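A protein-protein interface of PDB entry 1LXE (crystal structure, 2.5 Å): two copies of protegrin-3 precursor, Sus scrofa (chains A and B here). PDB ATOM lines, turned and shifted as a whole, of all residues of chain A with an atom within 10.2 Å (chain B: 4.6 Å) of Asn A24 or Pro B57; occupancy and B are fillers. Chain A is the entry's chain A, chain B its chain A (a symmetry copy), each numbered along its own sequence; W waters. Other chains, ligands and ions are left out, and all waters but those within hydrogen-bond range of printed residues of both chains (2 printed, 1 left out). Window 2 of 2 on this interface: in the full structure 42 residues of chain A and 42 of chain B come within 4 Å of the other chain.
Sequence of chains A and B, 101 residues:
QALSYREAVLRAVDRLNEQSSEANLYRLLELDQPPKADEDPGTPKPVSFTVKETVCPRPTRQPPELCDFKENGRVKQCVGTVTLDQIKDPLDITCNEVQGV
Of the 14 printed residues of chain A, 9 touch a printed residue of chain B. Along chain A the printed residues that touch a printed residue of chain B span positions 17 to 27. Among the printed residues, no Asp or Glu carboxylate lies within 4 Å of a Lys or Arg side-chain nitrogen of the other chain.
Water W1 lies within hydrogen-bond range of the guanidinium group (NH1) of Arg B58 (2.6 Å) and the side-chain carboxylate (OE2) of Glu A18 (3.4 Å). Water W2 bridges NE of Arg B58 and O of Glu A22.
NH1 of Arg B58 lies within hydrogen-bond range of O of Asn A17 (3.0 Å). The backbone carbonyl oxygen (O) of Ser A20 is in hydrogen-bond range of the guanidinium group (NE) of Arg B58, 2.8 Å away. The backbone carbonyl oxygen (O) of Glu A22 sits close to the guanidinium group (NE) of Arg B58. O of Ala A23 sits at hydrogen-bond distance from N of Arg B58 (2.7 Å). ND2 of Asn A24 sits at hydrogen-bond distance from OE2 of Glu B53. The side-chain amide oxygen (OD1) of Asn A24 lies close to the backbone carbonyl oxygen (O) of Cys B56 (3.2 Å). The backbone NH (N) of Thr B54 lies within hydrogen-bond range of the backbone carbonyl oxygen (O) of Leu A25, 3.0 Å away. The backbone carbonyl oxygen (O) of Cys B56 sits at hydrogen-bond distance from the backbone NH (N) of Leu A25, at 3.0 Å.
ND2 of Asn A17 is in hydrogen-bond range of O of Val A13. OD1 of Asn A17 is in hydrogen-bond range of N of Tyr A26 (2.9 Å). OG of Ser A20 lies within hydrogen-bond range of N of Glu A22 (3.1 Å). OE2 of Glu A22 lies within hydrogen-bond range of OH of Tyr A26 (2.8 Å). The side-chain hydroxyl of Thr B54 lies within hydrogen-bond range of the backbone NH of Cys B56 (3.1 Å). The backbone carbonyl oxygen of Pro B57 sits at hydrogen-bond distance from the side-chain hydroxyl of Thr B60 (2.6 Å).
Among the printed residues, merely in contact across the chains: Leu A25 with Arg B58 (3.3 Å), Tyr A26 with Glu B53 (3.4 Å), Glu A18 with Arg B58 (3.5 Å), Asn A24 with Thr B54 (3.5 Å), Ala A23 with Pro B57 (3.5 Å), Asn A24 with Arg B58 (3.6 Å), Asn A24 with Pro B57 (3.6 Å), Arg A27 with Thr B54 (3.7 Å) and Leu A25 with Glu B53 (3.95 Å).
Asn A24 touches just these residues of chain B: Glu B53, Thr B54, Cys B56, Pro B57 and Arg B58. Of chain A, only Ala A23 and Asn A24 come within 4 Å of Pro B57. Of chain A, only Asn A24 and Leu A25 come within 4 Å of Cys B56. No residue of chain A comes within 4 Å of Thr B60. Printed residues of chain B within 4 Å of Ser A20: Arg B58. Of the printed residues of chain B, Asn A17 touches Arg B58. Of the printed residues of chain B, Arg A27 touches Thr B54. Printed residues of chain B within 4 Å of Tyr A26: Glu B53 (3.4 Å). Of the printed residues of chain A, Thr B54 touches Asn A24 (3.5 Å), Leu A25 (3.0 Å) and Arg A27 (3.7 Å). The nearest residue of chain A that does not touch Pro B57 is Leu A25 (4.3 Å).
No position is printed for both chains.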
ATOM      1  N   VAL A  13      -8.553  24.006   3.748  1.00  0.00           N
ATOM      2  CA  VAL A  13      -9.424  22.865   3.485  1.00  0.00           C
ATOM      3  C   VAL A  13      -8.590  21.804   2.763  1.00  0.00           C
ATOM      4  O   VAL A  13      -8.734  20.617   3.021  1.00  0.00           O
ATOM      5  CB  VAL A  13     -10.678  23.261   2.616  1.00  0.00           C
ATOM      6  CG1 VAL A  13     -11.472  22.016   2.222  1.00  0.00           C
ATOM      7  CG2 VAL A  13     -11.574  24.215   3.400  1.00  0.00           C
ATOM      8  N   ASP A  14      -7.707  22.237   1.868  1.00  0.00           N
ATOM      9  CA  ASP A  14      -6.858  21.289   1.155  1.00  0.00           C
ATOM     10  C   ASP A  14      -5.957  20.536   2.132  1.00  0.00           C
ATOM     11  O   ASP A  14      -5.735  19.326   1.995  1.00  0.00           O
ATOM     12  CB  ASP A  14      -5.985  21.996   0.125  1.00  0.00           C
ATOM     13  CG  ASP A  14      -6.707  22.251  -1.165  1.00  0.00           C
ATOM     14  OD1 ASP A  14      -7.267  21.300  -1.722  1.00  0.00           O
ATOM     15  OD2 ASP A  14      -6.710  23.398  -1.634  1.00  0.00           O
ATOM     16  N   LEU A  16      -6.611  20.086   5.310  1.00  0.00           N
ATOM     17  CA  LEU A  16      -7.428  19.217   6.145  1.00  0.00           C
ATOM     18  C   LEU A  16      -7.654  17.909   5.398  1.00  0.00           C
ATOM     19  O   LEU A  16      -7.756  16.857   6.009  1.00  0.00           O
ATOM     20  CB  LEU A  16      -8.775  19.857   6.488  1.00  0.00           C
ATOM     21  CG  LEU A  16      -9.869  18.806   6.747  1.00  0.00           C
ATOM     22  CD1 LEU A  16      -9.623  18.102   8.086  1.00  0.00           C
ATOM     23  CD2 LEU A  16     -11.257  19.457   6.698  1.00  0.00           C
ATOM     24  N   ASN A  17      -7.726  17.970   4.073  1.00  0.00           N
ATOM     25  CA  ASN A  17      -7.939  16.752   3.293  1.00  0.00           C
ATOM     26  C   ASN A  17      -6.664  15.916   3.201  1.00  0.00           C
ATOM     27  O   ASN A  17      -6.714  14.709   2.946  1.00  0.00           O
ATOM     28  CB  ASN A  17      -8.462  17.089   1.885  1.00  0.00           C
ATOM     29  CG  ASN A  17      -9.946  17.432   1.878  1.00  0.00           C
ATOM     30  OD1 ASN A  17     -10.732  16.823   2.601  1.00  0.00           O
ATOM     31  ND2 ASN A  17     -10.337  18.393   1.043  1.00  0.00           N
ATOM     32  N   GLU A  18      -5.523  16.567   3.412  1.00  0.00           N
ATOM     33  CA  GLU A  18      -4.233  15.886   3.363  1.00  0.00           C
ATOM     34  C   GLU A  18      -4.031  15.122   4.668  1.00  0.00           C
ATOM     35  O   GLU A  18      -3.780  13.918   4.661  1.00  0.00           O
ATOM     36  CB  GLU A  18      -3.111  16.902   3.173  1.00  0.00           C
ATOM     37  CG  GLU A  18      -2.119  16.522   2.095  1.00  0.00           C
ATOM     38  CD  GLU A  18      -2.790  16.299   0.747  1.00  0.00           C
ATOM     39  OE1 GLU A  18      -3.496  17.219   0.279  1.00  0.00           O
ATOM     40  OE2 GLU A  18      -2.609  15.208   0.155  1.00  0.00           O
ATOM     41  N   GLN A  19      -4.162  15.836   5.781  1.00  0.00           N
ATOM     42  CA  GLN A  19      -4.013  15.265   7.109  1.00  0.00           C
ATOM     43  C   GLN A  19      -5.344  14.709   7.584  1.00  0.00           C
ATOM     44  O   GLN A  19      -5.894  15.156   8.590  1.00  0.00           O
ATOM     45  CB  GLN A  19      -3.535  16.335   8.088  1.00  0.00           C
ATOM     46  CG  GLN A  19      -2.130  16.844   7.817  1.00  0.00           C
ATOM     47  CD  GLN A  19      -1.701  17.914   8.808  1.00  0.00           C
ATOM     48  OE1 GLN A  19      -2.268  19.007   8.840  1.00  0.00           O
ATOM     49  NE2 GLN A  19      -0.702  17.600   9.628  1.00  0.00           N
ATOM     50  N   SER A  20      -5.870  13.742   6.849  1.00  0.00           N
ATOM     51  CA  SER A  20      -7.147  13.134   7.205  1.00  0.00           C
ATOM     52  C   SER A  20      -7.173  11.670   6.803  1.00  0.00           C
ATOM     53  O   SER A  20      -6.720  11.309   5.716  1.00  0.00           O
ATOM     54  CB  SER A  20      -8.306  13.867   6.521  1.00  0.00           C
ATOM     55  OG  SER A  20      -9.553  13.257   6.820  1.00  0.00           O
ATOM     56  N   SER A  21      -7.702  10.833   7.685  1.00  0.00           N
ATOM     57  CA  SER A  21      -7.789   9.402   7.418  1.00  0.00           C
ATOM     58  C   SER A  21      -9.151   9.105   6.810  1.00  0.00           C
ATOM     59  O   SER A  21      -9.456   7.963   6.466  1.00  0.00           O
ATOM     60  CB  SER A  21      -7.624   8.616   8.715  1.00  0.00           C
ATOM     61  OG  SER A  21      -8.661   8.939   9.629  1.00  0.00           O
ATOM     62  N   GLU A  22      -9.964  10.150   6.689  1.00  0.00           N
ATOM     63  CA  GLU A  22     -11.304  10.030   6.134  1.00  0.00           C
ATOM     64  C   GLU A  22     -11.259   9.394   4.748  1.00  0.00           C
ATOM     65  O   GLU A  22     -10.219   9.367   4.088  1.00  0.00           O
ATOM     66  CB  GLU A  22     -11.965  11.407   6.043  1.00  0.00           C
ATOM     67  CG  GLU A  22     -13.446  11.418   6.392  1.00  0.00           C
ATOM     68  CD  GLU A  22     -13.687  11.431   7.890  1.00  0.00           C
ATOM     69  OE1 GLU A  22     -13.136  10.556   8.585  1.00  0.00           O
ATOM     70  OE2 GLU A  22     -14.425  12.313   8.374  1.00  0.00           O
ATOM     71  N   ALA A  23     -12.402   8.895   4.304  1.00  0.00           N
ATOM     72  CA  ALA A  23     -12.483   8.248   3.016  1.00  0.00           C
ATOM     73  C   ALA A  23     -12.788   9.199   1.864  1.00  0.00           C
ATOM     74  O   ALA A  23     -12.422   8.920   0.727  1.00  0.00           O
ATOM     75  CB  ALA A  23     -13.518   7.151   3.068  1.00  0.00           C
ATOM     76  N   ASN A  24     -13.469  10.304   2.133  1.00  0.00           N
ATOM     77  CA  ASN A  24     -13.779  11.241   1.055  1.00  0.00           C
ATOM     78  C   ASN A  24     -13.222  12.632   1.322  1.00  0.00           C
ATOM     79  O   ASN A  24     -12.873  12.966   2.449  1.00  0.00           O
ATOM     80  CB  ASN A  24     -15.290  11.365   0.824  1.00  0.00           C
ATOM     81  CG  ASN A  24     -15.937  10.059   0.410  1.00  0.00           C
ATOM     82  OD1 ASN A  24     -15.556   9.448  -0.591  1.00  0.00           O
ATOM     83  ND2 ASN A  24     -16.930   9.627   1.179  1.00  0.00           N
ATOM     84  N   LEU A  25     -13.127  13.432   0.269  1.00  0.00           N
ATOM     85  CA  LEU A  25     -12.646  14.794   0.409  1.00  0.00           C
ATOM     86  C   LEU A  25     -13.799  15.620   0.932  1.00  0.00           C
ATOM     87  O   LEU A  25     -14.953  15.257   0.746  1.00  0.00           O
ATOM     88  CB  LEU A  25     -12.234  15.381  -0.944  1.00  0.00           C
ATOM     89  CG  LEU A  25     -11.019  14.879  -1.710  1.00  0.00           C
ATOM     90  CD1 LEU A  25     -10.980  15.627  -3.042  1.00  0.00           C
ATOM     91  CD2 LEU A  25      -9.739  15.107  -0.910  1.00  0.00           C
ATOM     92  N   TYR A  26     -13.485  16.719   1.601  1.00  0.00           N
ATOM     93  CA  TYR A  26     -14.517  17.640   2.076  1.00  0.00           C
ATOM     94  C   TYR A  26     -14.336  18.936   1.294  1.00  0.00           C
ATOM     95  O   TYR A  26     -13.263  19.195   0.778  1.00  0.00           O
ATOM     96  CB  TYR A  26     -14.350  17.949   3.567  1.00  0.00           C
ATOM     97  CG  TYR A  26     -14.877  16.870   4.487  1.00  0.00           C
ATOM     98  CD1 TYR A  26     -14.151  15.700   4.717  1.00  0.00           C
ATOM     99  CD2 TYR A  26     -16.106  17.025   5.128  1.00  0.00           C
ATOM    100  CE1 TYR A  26     -14.637  14.706   5.568  1.00  0.00           C
ATOM    101  CE2 TYR A  26     -16.595  16.059   5.974  1.00  0.00           C
ATOM    102  CZ  TYR A  26     -15.862  14.895   6.198  1.00  0.00           C
ATOM    103  OH  TYR A  26     -16.352  13.944   7.065  1.00  0.00           O
ATOM    104  N   ARG A  27     -15.384  19.735   1.164  1.00  0.00           N
ATOM    105  CA  ARG A  27     -15.231  21.007   0.501  1.00  0.00           C
ATOM    106  C   ARG A  27     -15.955  22.067   1.317  1.00  0.00           C
ATOM    107  O   ARG A  27     -16.779  21.744   2.163  1.00  0.00           O
ATOM    108  CB  ARG A  27     -15.746  20.964  -0.948  1.00  0.00           C
ATOM    109  CG  ARG A  27     -17.237  21.004  -1.104  1.00  0.00           C
ATOM    110  CD  ARG A  27     -17.647  20.883  -2.574  1.00  0.00           C
ATOM    111  NE  ARG A  27     -17.928  22.180  -3.160  1.00  0.00           N
ATOM    112  CZ  ARG A  27     -18.793  22.379  -4.149  1.00  0.00           C
ATOM    113  NH1 ARG A  27     -19.456  21.364  -4.673  1.00  0.00           N
ATOM    114  NH2 ARG A  27     -19.028  23.602  -4.584  1.00  0.00           N
ATOM    115  N   GLU B  53     -19.002  16.658   3.480  1.00  0.00           N
ATOM    116  CA  GLU B  53     -18.417  15.539   2.766  1.00  0.00           C
ATOM    117  C   GLU B  53     -18.857  15.514   1.303  1.00  0.00           C
ATOM    118  O   GLU B  53     -20.031  15.710   1.002  1.00  0.00           O
ATOM    119  CB  GLU B  53     -18.838  14.229   3.457  1.00  0.00           C
ATOM    120  CG  GLU B  53     -17.937  13.028   3.194  1.00  0.00           C
ATOM    121  CD  GLU B  53     -18.546  11.719   3.679  1.00  0.00           C
ATOM    122  OE1 GLU B  53     -19.523  11.754   4.459  1.00  0.00           O
ATOM    123  OE2 GLU B  53     -18.046  10.648   3.287  1.00  0.00           O
ATOM    124  N   THR B  54     -17.923  15.277   0.382  1.00  0.00           N
ATOM    125  CA  THR B  54     -18.325  15.193  -1.023  1.00  0.00           C
ATOM    126  C   THR B  54     -18.347  13.737  -1.487  1.00  0.00           C
ATOM    127  O   THR B  54     -18.124  12.814  -0.704  1.00  0.00           O
ATOM    128  CB  THR B  54     -17.403  16.006  -1.963  1.00  0.00           C
ATOM    129  OG1 THR B  54     -16.242  15.233  -2.286  1.00  0.00           O
ATOM    130  CG2 THR B  54     -17.002  17.358  -1.309  1.00  0.00           C
ATOM    131  N   VAL B  55     -18.624  13.525  -2.764  1.00  0.00           N
ATOM    132  CA  VAL B  55     -18.671  12.167  -3.296  1.00  0.00           C
ATOM    133  C   VAL B  55     -17.326  11.682  -3.837  1.00  0.00           C
ATOM    134  O   VAL B  55     -17.238  10.567  -4.338  1.00  0.00           O
ATOM    135  CB  VAL B  55     -19.719  12.052  -4.438  1.00  0.00           C
ATOM    136  CG1 VAL B  55     -21.126  12.273  -3.888  1.00  0.00           C
ATOM    137  CG2 VAL B  55     -19.398  13.066  -5.540  1.00  0.00           C
ATOM    138  N   CYS B  56     -16.285  12.509  -3.732  1.00  0.00           N
ATOM    139  CA  CYS B  56     -14.957  12.156  -4.238  1.00  0.00           C
ATOM    140  C   CYS B  56     -14.106  11.367  -3.236  1.00  0.00           C
ATOM    141  O   CYS B  56     -13.978  11.760  -2.083  1.00  0.00           O
ATOM    142  CB  CYS B  56     -14.178  13.434  -4.659  1.00  0.00           C
ATOM    143  SG  CYS B  56     -14.755  14.307  -6.172  1.00  0.00           S
ATOM    144  N   PRO B  57     -13.520  10.236  -3.666  1.00  0.00           N
ATOM    145  CA  PRO B  57     -12.670   9.425  -2.776  1.00  0.00           C
ATOM    146  C   PRO B  57     -11.453  10.276  -2.407  1.00  0.00           C
ATOM    147  O   PRO B  57     -10.836  10.863  -3.293  1.00  0.00           O
ATOM    148  CB  PRO B  57     -12.285   8.239  -3.650  1.00  0.00           C
ATOM    149  CG  PRO B  57     -13.439   8.121  -4.604  1.00  0.00           C
ATOM    150  CD  PRO B  57     -13.739   9.548  -4.951  1.00  0.00           C
ATOM    151  N   ARG B  58     -11.102  10.319  -1.119  1.00  0.00           N
ATOM    152  CA  ARG B  58      -9.994  11.151  -0.620  1.00  0.00           C
ATOM    153  C   ARG B  58      -8.676  11.247  -1.390  1.00  0.00           C
ATOM    154  O   ARG B  58      -8.092  12.320  -1.472  1.00  0.00           O
ATOM    155  CB  ARG B  58      -9.669  10.799   0.836  1.00  0.00           C
ATOM    156  CG  ARG B  58      -8.744  11.825   1.492  1.00  0.00           C
ATOM    157  CD  ARG B  58      -8.501  11.544   2.963  1.00  0.00           C
ATOM    158  NE  ARG B  58      -7.473  10.530   3.177  1.00  0.00           N
ATOM    159  CZ  ARG B  58      -6.178  10.730   2.980  1.00  0.00           C
ATOM    160  NH1 ARG B  58      -5.740  11.912   2.564  1.00  0.00           N
ATOM    161  NH2 ARG B  58      -5.316   9.749   3.208  1.00  0.00           N
ATOM    162  N   PRO B  59      -8.178  10.136  -1.943  1.00  0.00           N
ATOM    163  CA  PRO B  59      -6.913  10.217  -2.678  1.00  0.00           C
ATOM    164  C   PRO B  59      -7.078  10.722  -4.102  1.00  0.00           C
ATOM    165  O   PRO B  59      -6.653  10.058  -5.044  1.00  0.00           O
ATOM    166  CB  PRO B  59      -6.427   8.782  -2.654  1.00  0.00           C
ATOM    167  CG  PRO B  59      -7.715   8.035  -2.807  1.00  0.00           C
ATOM    168  CD  PRO B  59      -8.613   8.734  -1.813  1.00  0.00           C
ATOM    169  N   THR B  60      -7.679  11.892  -4.266  1.00  0.00           N
ATOM    170  CA  THR B  60      -7.899  12.431  -5.601  1.00  0.00           C
ATOM    171  C   THR B  60      -7.148  13.725  -5.863  1.00  0.00           C
ATOM    172  O   THR B  60      -7.010  14.562  -4.973  1.00  0.00           O
ATOM    173  CB  THR B  60      -9.392  12.666  -5.853  1.00  0.00           C
ATOM    174  OG1 THR B  60     -10.096  11.426  -5.715  1.00  0.00           O
ATOM    175  CG2 THR B  60      -9.614  13.202  -7.247  1.00  0.00           C
HETATM  176  O   HOH W   1      -4.747  12.628   0.248  1.00  0.00           O
HETATM  177  O   HOH W   2      -7.663   7.883   3.038  1.00  0.00           O
